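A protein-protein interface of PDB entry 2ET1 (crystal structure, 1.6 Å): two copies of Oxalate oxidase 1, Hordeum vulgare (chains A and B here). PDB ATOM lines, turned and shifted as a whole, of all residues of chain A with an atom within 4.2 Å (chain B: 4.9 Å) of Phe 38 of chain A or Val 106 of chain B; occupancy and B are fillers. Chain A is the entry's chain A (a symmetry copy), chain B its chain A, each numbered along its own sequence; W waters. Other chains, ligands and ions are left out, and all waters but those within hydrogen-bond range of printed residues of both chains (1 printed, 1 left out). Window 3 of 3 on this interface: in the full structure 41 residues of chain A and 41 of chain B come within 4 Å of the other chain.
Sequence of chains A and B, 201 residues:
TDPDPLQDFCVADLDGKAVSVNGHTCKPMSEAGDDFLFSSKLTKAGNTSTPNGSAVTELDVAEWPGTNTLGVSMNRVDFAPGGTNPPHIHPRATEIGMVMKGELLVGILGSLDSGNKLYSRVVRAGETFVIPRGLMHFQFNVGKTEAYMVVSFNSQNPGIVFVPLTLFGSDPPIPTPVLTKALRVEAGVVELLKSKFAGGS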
ATOM      1  N   ASP A  35      -2.265 -27.868  10.351  1.00  0.00           N
ATOM      2  CA  ASP A  35      -0.981 -27.280  10.765  1.00  0.00           C
ATOM      3  C   ASP A  35      -0.966 -25.818  11.229  1.00  0.00           C
ATOM      4  O   ASP A  35       0.116 -25.272  11.487  1.00  0.00           O
ATOM      5  CB  ASP A  35       0.099 -27.526   9.685  1.00  0.00           C
ATOM      6  CG  ASP A  35       0.094 -26.498   8.557  1.00  0.00           C
ATOM      7  OD1 ASP A  35      -0.743 -25.569   8.531  1.00  0.00           O
ATOM      8  OD2 ASP A  35       0.967 -26.619   7.664  1.00  0.00           O
ATOM      9  N   PHE A  36      -2.140 -25.188  11.342  1.00  0.00           N
ATOM     10  CA  PHE A  36      -2.168 -23.737  11.545  1.00  0.00           C
ATOM     11  C   PHE A  36      -1.684 -23.274  12.930  1.00  0.00           C
ATOM     12  O   PHE A  36      -1.270 -22.123  13.083  1.00  0.00           O
ATOM     13  CB  PHE A  36      -3.561 -23.156  11.228  1.00  0.00           C
ATOM     14  CG  PHE A  36      -4.672 -23.748  12.059  1.00  0.00           C
ATOM     15  CD1 PHE A  36      -5.010 -23.192  13.310  1.00  0.00           C
ATOM     16  CD2 PHE A  36      -5.398 -24.857  11.607  1.00  0.00           C
ATOM     17  CE1 PHE A  36      -6.045 -23.742  14.081  1.00  0.00           C
ATOM     18  CE2 PHE A  36      -6.421 -25.409  12.363  1.00  0.00           C
ATOM     19  CZ  PHE A  36      -6.750 -24.846  13.620  1.00  0.00           C
ATOM     20  N   LEU A  37      -1.732 -24.163  13.928  1.00  0.00           N
ATOM     21  CA  LEU A  37      -1.253 -23.822  15.291  1.00  0.00           C
ATOM     22  C   LEU A  37       0.268 -23.946  15.475  1.00  0.00           C
ATOM     23  O   LEU A  37       0.765 -23.780  16.593  1.00  0.00           O
ATOM     24  CB  LEU A  37      -1.968 -24.675  16.351  1.00  0.00           C
ATOM     25  CG  LEU A  37      -3.485 -24.512  16.456  1.00  0.00           C
ATOM     26  CD1 LEU A  37      -4.106 -25.601  17.315  1.00  0.00           C
ATOM     27  CD2 LEU A  37      -3.815 -23.117  17.010  1.00  0.00           C
ATOM     28  N   PHE A  38       1.001 -24.220  14.384  1.00  0.00           N
ATOM     29  CA  PHE A  38       2.450 -24.495  14.433  1.00  0.00           C
ATOM     30  C   PHE A  38       3.235 -23.641  13.418  1.00  0.00           C
ATOM     31  O   PHE A  38       2.682 -23.234  12.381  1.00  0.00           O
ATOM     32  CB  PHE A  38       2.694 -25.993  14.143  1.00  0.00           C
ATOM     33  CG  PHE A  38       1.970 -26.923  15.093  1.00  0.00           C
ATOM     34  CD1 PHE A  38       0.757 -27.533  14.727  1.00  0.00           C
ATOM     35  CD2 PHE A  38       2.498 -27.185  16.357  1.00  0.00           C
ATOM     36  CE1 PHE A  38       0.086 -28.389  15.621  1.00  0.00           C
ATOM     37  CE2 PHE A  38       1.829 -28.035  17.257  1.00  0.00           C
ATOM     38  CZ  PHE A  38       0.616 -28.631  16.885  1.00  0.00           C
ATOM     39  N   SER A  39       4.519 -23.395  13.701  1.00  0.00           N
ATOM     40  CA  SER A  39       5.422 -22.732  12.733  1.00  0.00           C
ATOM     41  C   SER A  39       6.874 -23.175  12.889  1.00  0.00           C
ATOM     42  O   SER A  39       7.292 -23.618  13.972  1.00  0.00           O
ATOM     43  CB  SER A  39       5.341 -21.203  12.859  1.00  0.00           C
ATOM     44  OG  SER A  39       6.070 -20.508  11.841  1.00  0.00           O
ATOM     45  N   TRP A  64       2.173 -15.555  10.768  1.00  0.00           N
ATOM     46  CA  TRP A  64       1.599 -16.728  11.453  1.00  0.00           C
ATOM     47  C   TRP A  64       0.080 -16.536  11.587  1.00  0.00           C
ATOM     48  O   TRP A  64      -0.411 -16.109  12.642  1.00  0.00           O
ATOM     49  CB  TRP A  64       2.237 -16.934  12.843  1.00  0.00           C
ATOM     50  CG  TRP A  64       2.026 -18.296  13.461  1.00  0.00           C
ATOM     51  CD1 TRP A  64       1.348 -19.364  12.920  1.00  0.00           C
ATOM     52  CD2 TRP A  64       2.549 -18.754  14.714  1.00  0.00           C
ATOM     53  NE1 TRP A  64       1.390 -20.445  13.778  1.00  0.00           N
ATOM     54  CE2 TRP A  64       2.138 -20.103  14.879  1.00  0.00           C
ATOM     55  CE3 TRP A  64       3.325 -18.156  15.722  1.00  0.00           C
ATOM     56  CZ2 TRP A  64       2.466 -20.858  16.011  1.00  0.00           C
ATOM     57  CZ3 TRP A  64       3.653 -18.914  16.851  1.00  0.00           C
ATOM     58  CH2 TRP A  64       3.235 -20.251  16.976  1.00  0.00           C
ATOM     59  N   LEU B 104       9.393 -33.022  20.831  1.00  0.00           N
ATOM     60  CA  LEU B 104       8.155 -33.128  21.612  1.00  0.00           C
ATOM     61  C   LEU B 104       6.907 -33.295  20.735  1.00  0.00           C
ATOM     62  O   LEU B 104       6.634 -32.453  19.873  1.00  0.00           O
ATOM     63  CB  LEU B 104       7.978 -31.885  22.509  1.00  0.00           C
ATOM     64  CG  LEU B 104       8.966 -31.600  23.643  1.00  0.00           C
ATOM     65  CD1 LEU B 104       8.673 -30.229  24.259  1.00  0.00           C
ATOM     66  CD2 LEU B 104       8.857 -32.675  24.714  1.00  0.00           C
ATOM     67  N   LEU B 105       6.157 -34.373  20.950  1.00  0.00           N
ATOM     68  CA  LEU B 105       4.802 -34.463  20.401  1.00  0.00           C
ATOM     69  C   LEU B 105       3.927 -33.459  21.178  1.00  0.00           C
ATOM     70  O   LEU B 105       3.769 -33.588  22.400  1.00  0.00           O
ATOM     71  CB  LEU B 105       4.237 -35.888  20.531  1.00  0.00           C
ATOM     72  CG  LEU B 105       2.793 -36.036  20.015  1.00  0.00           C
ATOM     73  CD1 LEU B 105       2.730 -35.908  18.481  1.00  0.00           C
ATOM     74  CD2 LEU B 105       2.148 -37.349  20.493  1.00  0.00           C
ATOM     75  N   VAL B 106       3.387 -32.467  20.475  1.00  0.00           N
ATOM     76  CA  VAL B 106       2.522 -31.437  21.093  1.00  0.00           C
ATOM     77  C   VAL B 106       1.103 -31.627  20.564  1.00  0.00           C
ATOM     78  O   VAL B 106       0.897 -31.642  19.340  1.00  0.00           O
ATOM     79  CB  VAL B 106       3.023 -30.005  20.761  1.00  0.00           C
ATOM     80  CG1 VAL B 106       2.076 -28.940  21.356  1.00  0.00           C
ATOM     81  CG2 VAL B 106       4.451 -29.795  21.285  1.00  0.00           C
ATOM     82  N   GLY B 107       0.129 -31.783  21.467  1.00  0.00           N
ATOM     83  CA  GLY B 107      -1.276 -31.965  21.057  1.00  0.00           C
ATOM     84  C   GLY B 107      -2.202 -30.894  21.621  1.00  0.00           C
ATOM     85  O   GLY B 107      -2.080 -30.519  22.796  1.00  0.00           O
ATOM     86  N   ILE B 108      -3.131 -30.427  20.777  1.00  0.00           N
ATOM     87  CA  ILE B 108      -4.120 -29.397  21.135  1.00  0.00           C
ATOM     88  C   ILE B 108      -5.503 -29.899  20.748  1.00  0.00           C
ATOM     89  O   ILE B 108      -5.695 -30.376  19.623  1.00  0.00           O
ATOM     90  CB  ILE B 108      -3.845 -28.048  20.408  1.00  0.00           C
ATOM     91  CG1 ILE B 108      -2.417 -27.579  20.688  1.00  0.00           C
ATOM     92  CG2 ILE B 108      -4.849 -26.980  20.845  1.00  0.00           C
ATOM     93  CD1 ILE B 108      -1.527 -27.577  19.495  1.00  0.00           C
ATOM     94  N   TYR B 119      -5.318 -31.904  17.162  1.00  0.00           N
ATOM     95  CA  TYR B 119      -4.193 -31.498  16.302  1.00  0.00           C
ATOM     96  C   TYR B 119      -2.915 -31.841  17.021  1.00  0.00           C
ATOM     97  O   TYR B 119      -2.703 -31.419  18.161  1.00  0.00           O
ATOM     98  CB  TYR B 119      -4.184 -29.983  16.023  1.00  0.00           C
ATOM     99  CG  TYR B 119      -5.540 -29.432  15.770  1.00  0.00           C
ATOM    100  CD1 TYR B 119      -6.351 -29.130  16.853  1.00  0.00           C
ATOM    101  CD2 TYR B 119      -6.029 -29.235  14.484  1.00  0.00           C
ATOM    102  CE1 TYR B 119      -7.587 -28.663  16.713  1.00  0.00           C
ATOM    103  CE2 TYR B 119      -7.345 -28.722  14.323  1.00  0.00           C
ATOM    104  CZ  TYR B 119      -8.095 -28.448  15.484  1.00  0.00           C
ATOM    105  OH  TYR B 119      -9.386 -27.959  15.510  1.00  0.00           O
ATOM    106  N   SER B 120      -2.047 -32.589  16.359  1.00  0.00           N
ATOM    107  CA  SER B 120      -0.773 -32.957  16.981  1.00  0.00           C
ATOM    108  C   SER B 120       0.367 -33.057  15.984  1.00  0.00           C
ATOM    109  O   SER B 120       0.176 -33.511  14.852  1.00  0.00           O
ATOM    110  CB  SER B 120      -0.901 -34.229  17.827  1.00  0.00           C
ATOM    111  OG  SER B 120      -1.198 -35.372  17.023  1.00  0.00           O
ATOM    112  N   ARG B 121       1.554 -32.641  16.428  1.00  0.00           N
ATOM    113  CA  ARG B 121       2.743 -32.556  15.575  1.00  0.00           C
ATOM    114  C   ARG B 121       4.009 -32.769  16.419  1.00  0.00           C
ATOM    115  O   ARG B 121       4.065 -32.326  17.570  1.00  0.00           O
ATOM    116  CB  ARG B 121       2.784 -31.154  14.929  1.00  0.00           C
ATOM    117  CG  ARG B 121       3.885 -30.911  13.936  1.00  0.00           C
ATOM    118  CD  ARG B 121       3.893 -29.480  13.420  1.00  0.00           C
ATOM    119  NE  ARG B 121       4.876 -29.332  12.355  1.00  0.00           N
ATOM    120  CZ  ARG B 121       5.001 -28.276  11.558  1.00  0.00           C
ATOM    121  NH1 ARG B 121       4.207 -27.218  11.698  1.00  0.00           N
ATOM    122  NH2 ARG B 121       5.930 -28.275  10.610  1.00  0.00           N
ATOM    123  N   VAL B 123       7.359 -31.385  17.371  1.00  0.00           N
ATOM    124  CA  VAL B 123       7.953 -30.038  17.349  1.00  0.00           C
ATOM    125  C   VAL B 123       9.418 -30.096  17.829  1.00  0.00           C
ATOM    126  O   VAL B 123       9.711 -30.651  18.901  1.00  0.00           O
ATOM    127  CB  VAL B 123       7.119 -29.066  18.255  1.00  0.00           C
ATOM    128  CG1 VAL B 123       7.670 -27.649  18.223  1.00  0.00           C
ATOM    129  CG2 VAL B 123       5.641 -29.055  17.824  1.00  0.00           C
ATOM    130  N   THR B 128       7.707 -23.589  16.876  1.00  0.00           N
ATOM    131  CA  THR B 128       6.747 -22.936  17.805  1.00  0.00           C
ATOM    132  C   THR B 128       5.332 -23.509  17.701  1.00  0.00           C
ATOM    133  O   THR B 128       4.983 -24.128  16.694  1.00  0.00           O
ATOM    134  CB  THR B 128       6.716 -21.390  17.586  1.00  0.00           C
ATOM    135  OG1 THR B 128       6.449 -21.093  16.203  1.00  0.00           O
ATOM    136  CG2 THR B 128       8.074 -20.747  17.968  1.00  0.00           C
ATOM    137  N   PHE B 129       4.529 -23.282  18.753  1.00  0.00           N
ATOM    138  CA  PHE B 129       3.125 -23.719  18.803  1.00  0.00           C
ATOM    139  C   PHE B 129       2.280 -22.710  19.581  1.00  0.00           C
ATOM    140  O   PHE B 129       2.806 -21.900  20.360  1.00  0.00           O
ATOM    141  CB  PHE B 129       3.000 -25.127  19.429  1.00  0.00           C
ATOM    142  CG  PHE B 129       3.523 -25.225  20.854  1.00  0.00           C
ATOM    143  CD1 PHE B 129       2.697 -24.909  21.950  1.00  0.00           C
ATOM    144  CD2 PHE B 129       4.829 -25.649  21.103  1.00  0.00           C
ATOM    145  CE1 PHE B 129       3.181 -25.012  23.262  1.00  0.00           C
ATOM    146  CE2 PHE B 129       5.320 -25.763  22.413  1.00  0.00           C
ATOM    147  CZ  PHE B 129       4.491 -25.420  23.495  1.00  0.00           C
ATOM    148  N   ILE B 131      -1.483 -22.348  21.910  1.00  0.00           N
ATOM    149  CA  ILE B 131      -2.616 -23.004  22.581  1.00  0.00           C
ATOM    150  C   ILE B 131      -3.694 -21.960  22.913  1.00  0.00           C
ATOM    151  O   ILE B 131      -3.525 -21.165  23.844  1.00  0.00           O
ATOM    152  CB  ILE B 131      -2.213 -23.671  23.937  1.00  0.00           C
ATOM    153  CG1 ILE B 131      -0.813 -24.342  23.913  1.00  0.00           C
ATOM    154  CG2 ILE B 131      -3.325 -24.580  24.441  1.00  0.00           C
ATOM    155  CD1 ILE B 131      -0.708 -25.643  23.109  1.00  0.00           C
ATOM    156  N   PHE B 138      -1.364 -31.124  25.658  1.00  0.00           N
ATOM    157  CA  PHE B 138      -0.331 -31.954  26.305  1.00  0.00           C
ATOM    158  C   PHE B 138       0.974 -31.949  25.487  1.00  0.00           C
ATOM    159  O   PHE B 138       0.985 -31.546  24.312  1.00  0.00           O
ATOM    160  CB  PHE B 138      -0.820 -33.414  26.467  1.00  0.00           C
ATOM    161  CG  PHE B 138      -1.075 -34.130  25.154  1.00  0.00           C
ATOM    162  CD1 PHE B 138      -0.031 -34.778  24.479  1.00  0.00           C
ATOM    163  CD2 PHE B 138      -2.362 -34.156  24.603  1.00  0.00           C
ATOM    164  CE1 PHE B 138      -0.261 -35.442  23.251  1.00  0.00           C
ATOM    165  CE2 PHE B 138      -2.604 -34.817  23.375  1.00  0.00           C
ATOM    166  CZ  PHE B 138      -1.543 -35.442  22.702  1.00  0.00           C
ATOM    167  N   GLN B 139       2.063 -32.396  26.116  1.00  0.00           N
ATOM    168  CA  GLN B 139       3.340 -32.652  25.415  1.00  0.00           C
ATOM    169  C   GLN B 139       3.921 -33.992  25.868  1.00  0.00           C
ATOM    170  O   GLN B 139       3.719 -34.410  27.014  1.00  0.00           O
ATOM    171  CB  GLN B 139       4.381 -31.534  25.639  1.00  0.00           C
ATOM    172  CG  GLN B 139       3.959 -30.151  25.134  1.00  0.00           C
ATOM    173  CD  GLN B 139       3.199 -29.343  26.176  1.00  0.00           C
ATOM    174  OE1 GLN B 139       3.313 -29.591  27.384  1.00  0.00           O
ATOM    175  NE2 GLN B 139       2.454 -28.343  25.717  1.00  0.00           N
HETATM  176  O   HOH W   1       9.344 -21.202  14.647  1.00  0.00           O
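O of Ser 39 of chain A sits at hydrogen-bond distance from N of Thr 128 of chain B (2.9 Å).
Among the printed residues, merely in contact across the chains: Phe 38 of chain A with Arg 121 of chain B, Leu 37 of chain A with Phe 129 of chain B, Trp 64 of chain A with Thr 128 of chain B, Phe 38 of chain A with Thr 128 of chain B, Phe 38 of chain A with Ile 108 of chain B, Trp 64 of chain A with Phe 129 of chain B, Phe 38 of chain A with Phe 129 of chain B, Leu 37 of chain A with Ile 108 of chain B, Phe 38 of chain A with Val 106 of chain B, Phe 38 of chain A with Val 123 of chain B and Phe 36 of chain A with Tyr 119 of chain B.
Hydrophobic or aromatic side chains of chain A within 4 Å of the printed part of chain B: Phe 36, Leu 37, Phe 38 and Trp 64. Hydrophobic or aromatic side chains of chain B within 4 Å of the printed part of chain A: Ile 108, Tyr 119, Val 123 and Phe 129. Among the printed residues, 12 pairs touch across the chains.
O of Arg 121 of chain B lies within hydrogen-bond range of N of Val 106 of chain B (3.0 Å). The backbone carbonyl oxygen (O) of Tyr 119 of chain B is in hydrogen-bond range of the backbone NH (N) of Ile 108 of chain B, at 2.8 Å. O of Leu 104 of chain B is in hydrogen-bond range of N of Val 123 of chain B (2.8 Å). The backbone carbonyl oxygen (O) of Phe 36 of chain A sits at hydrogen-bond distance from the indole nitrogen (NE1) of Trp 64 of chain A, at 3.2 Å. O of Phe 38 of chain A lies within hydrogen-bond range of NE1 of Trp 64 of chain A.
No position is printed for both chains.
Water W1 bridges the backbone carbonyl oxygen of Ser 39 of chain A (3.2 Å) and the side-chain hydroxyl of Thr 128 of chain B (3.3 Å).
Of the printed residues of chain B, Phe 36 of chain A touches Tyr 119 (3.96 Å). Printed residues of chain B within 4 Å of Leu 37 of chain A: Ile 108 and Phe 129. Of the printed residues of chain B, Ser 39 of chain A touches Thr 128 (2.9 Å). Printed residues of chain B within 4 Å of Trp 64 of chain A: Thr 128 (3.4 Å) and Phe 129 (3.7 Å). Val 106 of chain B touches just one residue of chain A: Phe 38. Of the printed residues of chain A, Thr 128 of chain B touches Phe 38, Ser 39 and Trp 64. Ile 131 of chain B touches none of the printed residues of chain A. The nearest printed residue of chain A that does not touch Val 106 of chain B is Leu 37 of chain A (7.1 Å). The nearest printed residue of chain B that does not touch Leu 37 of chain A is Tyr 119 of chain B (4.2 Å).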
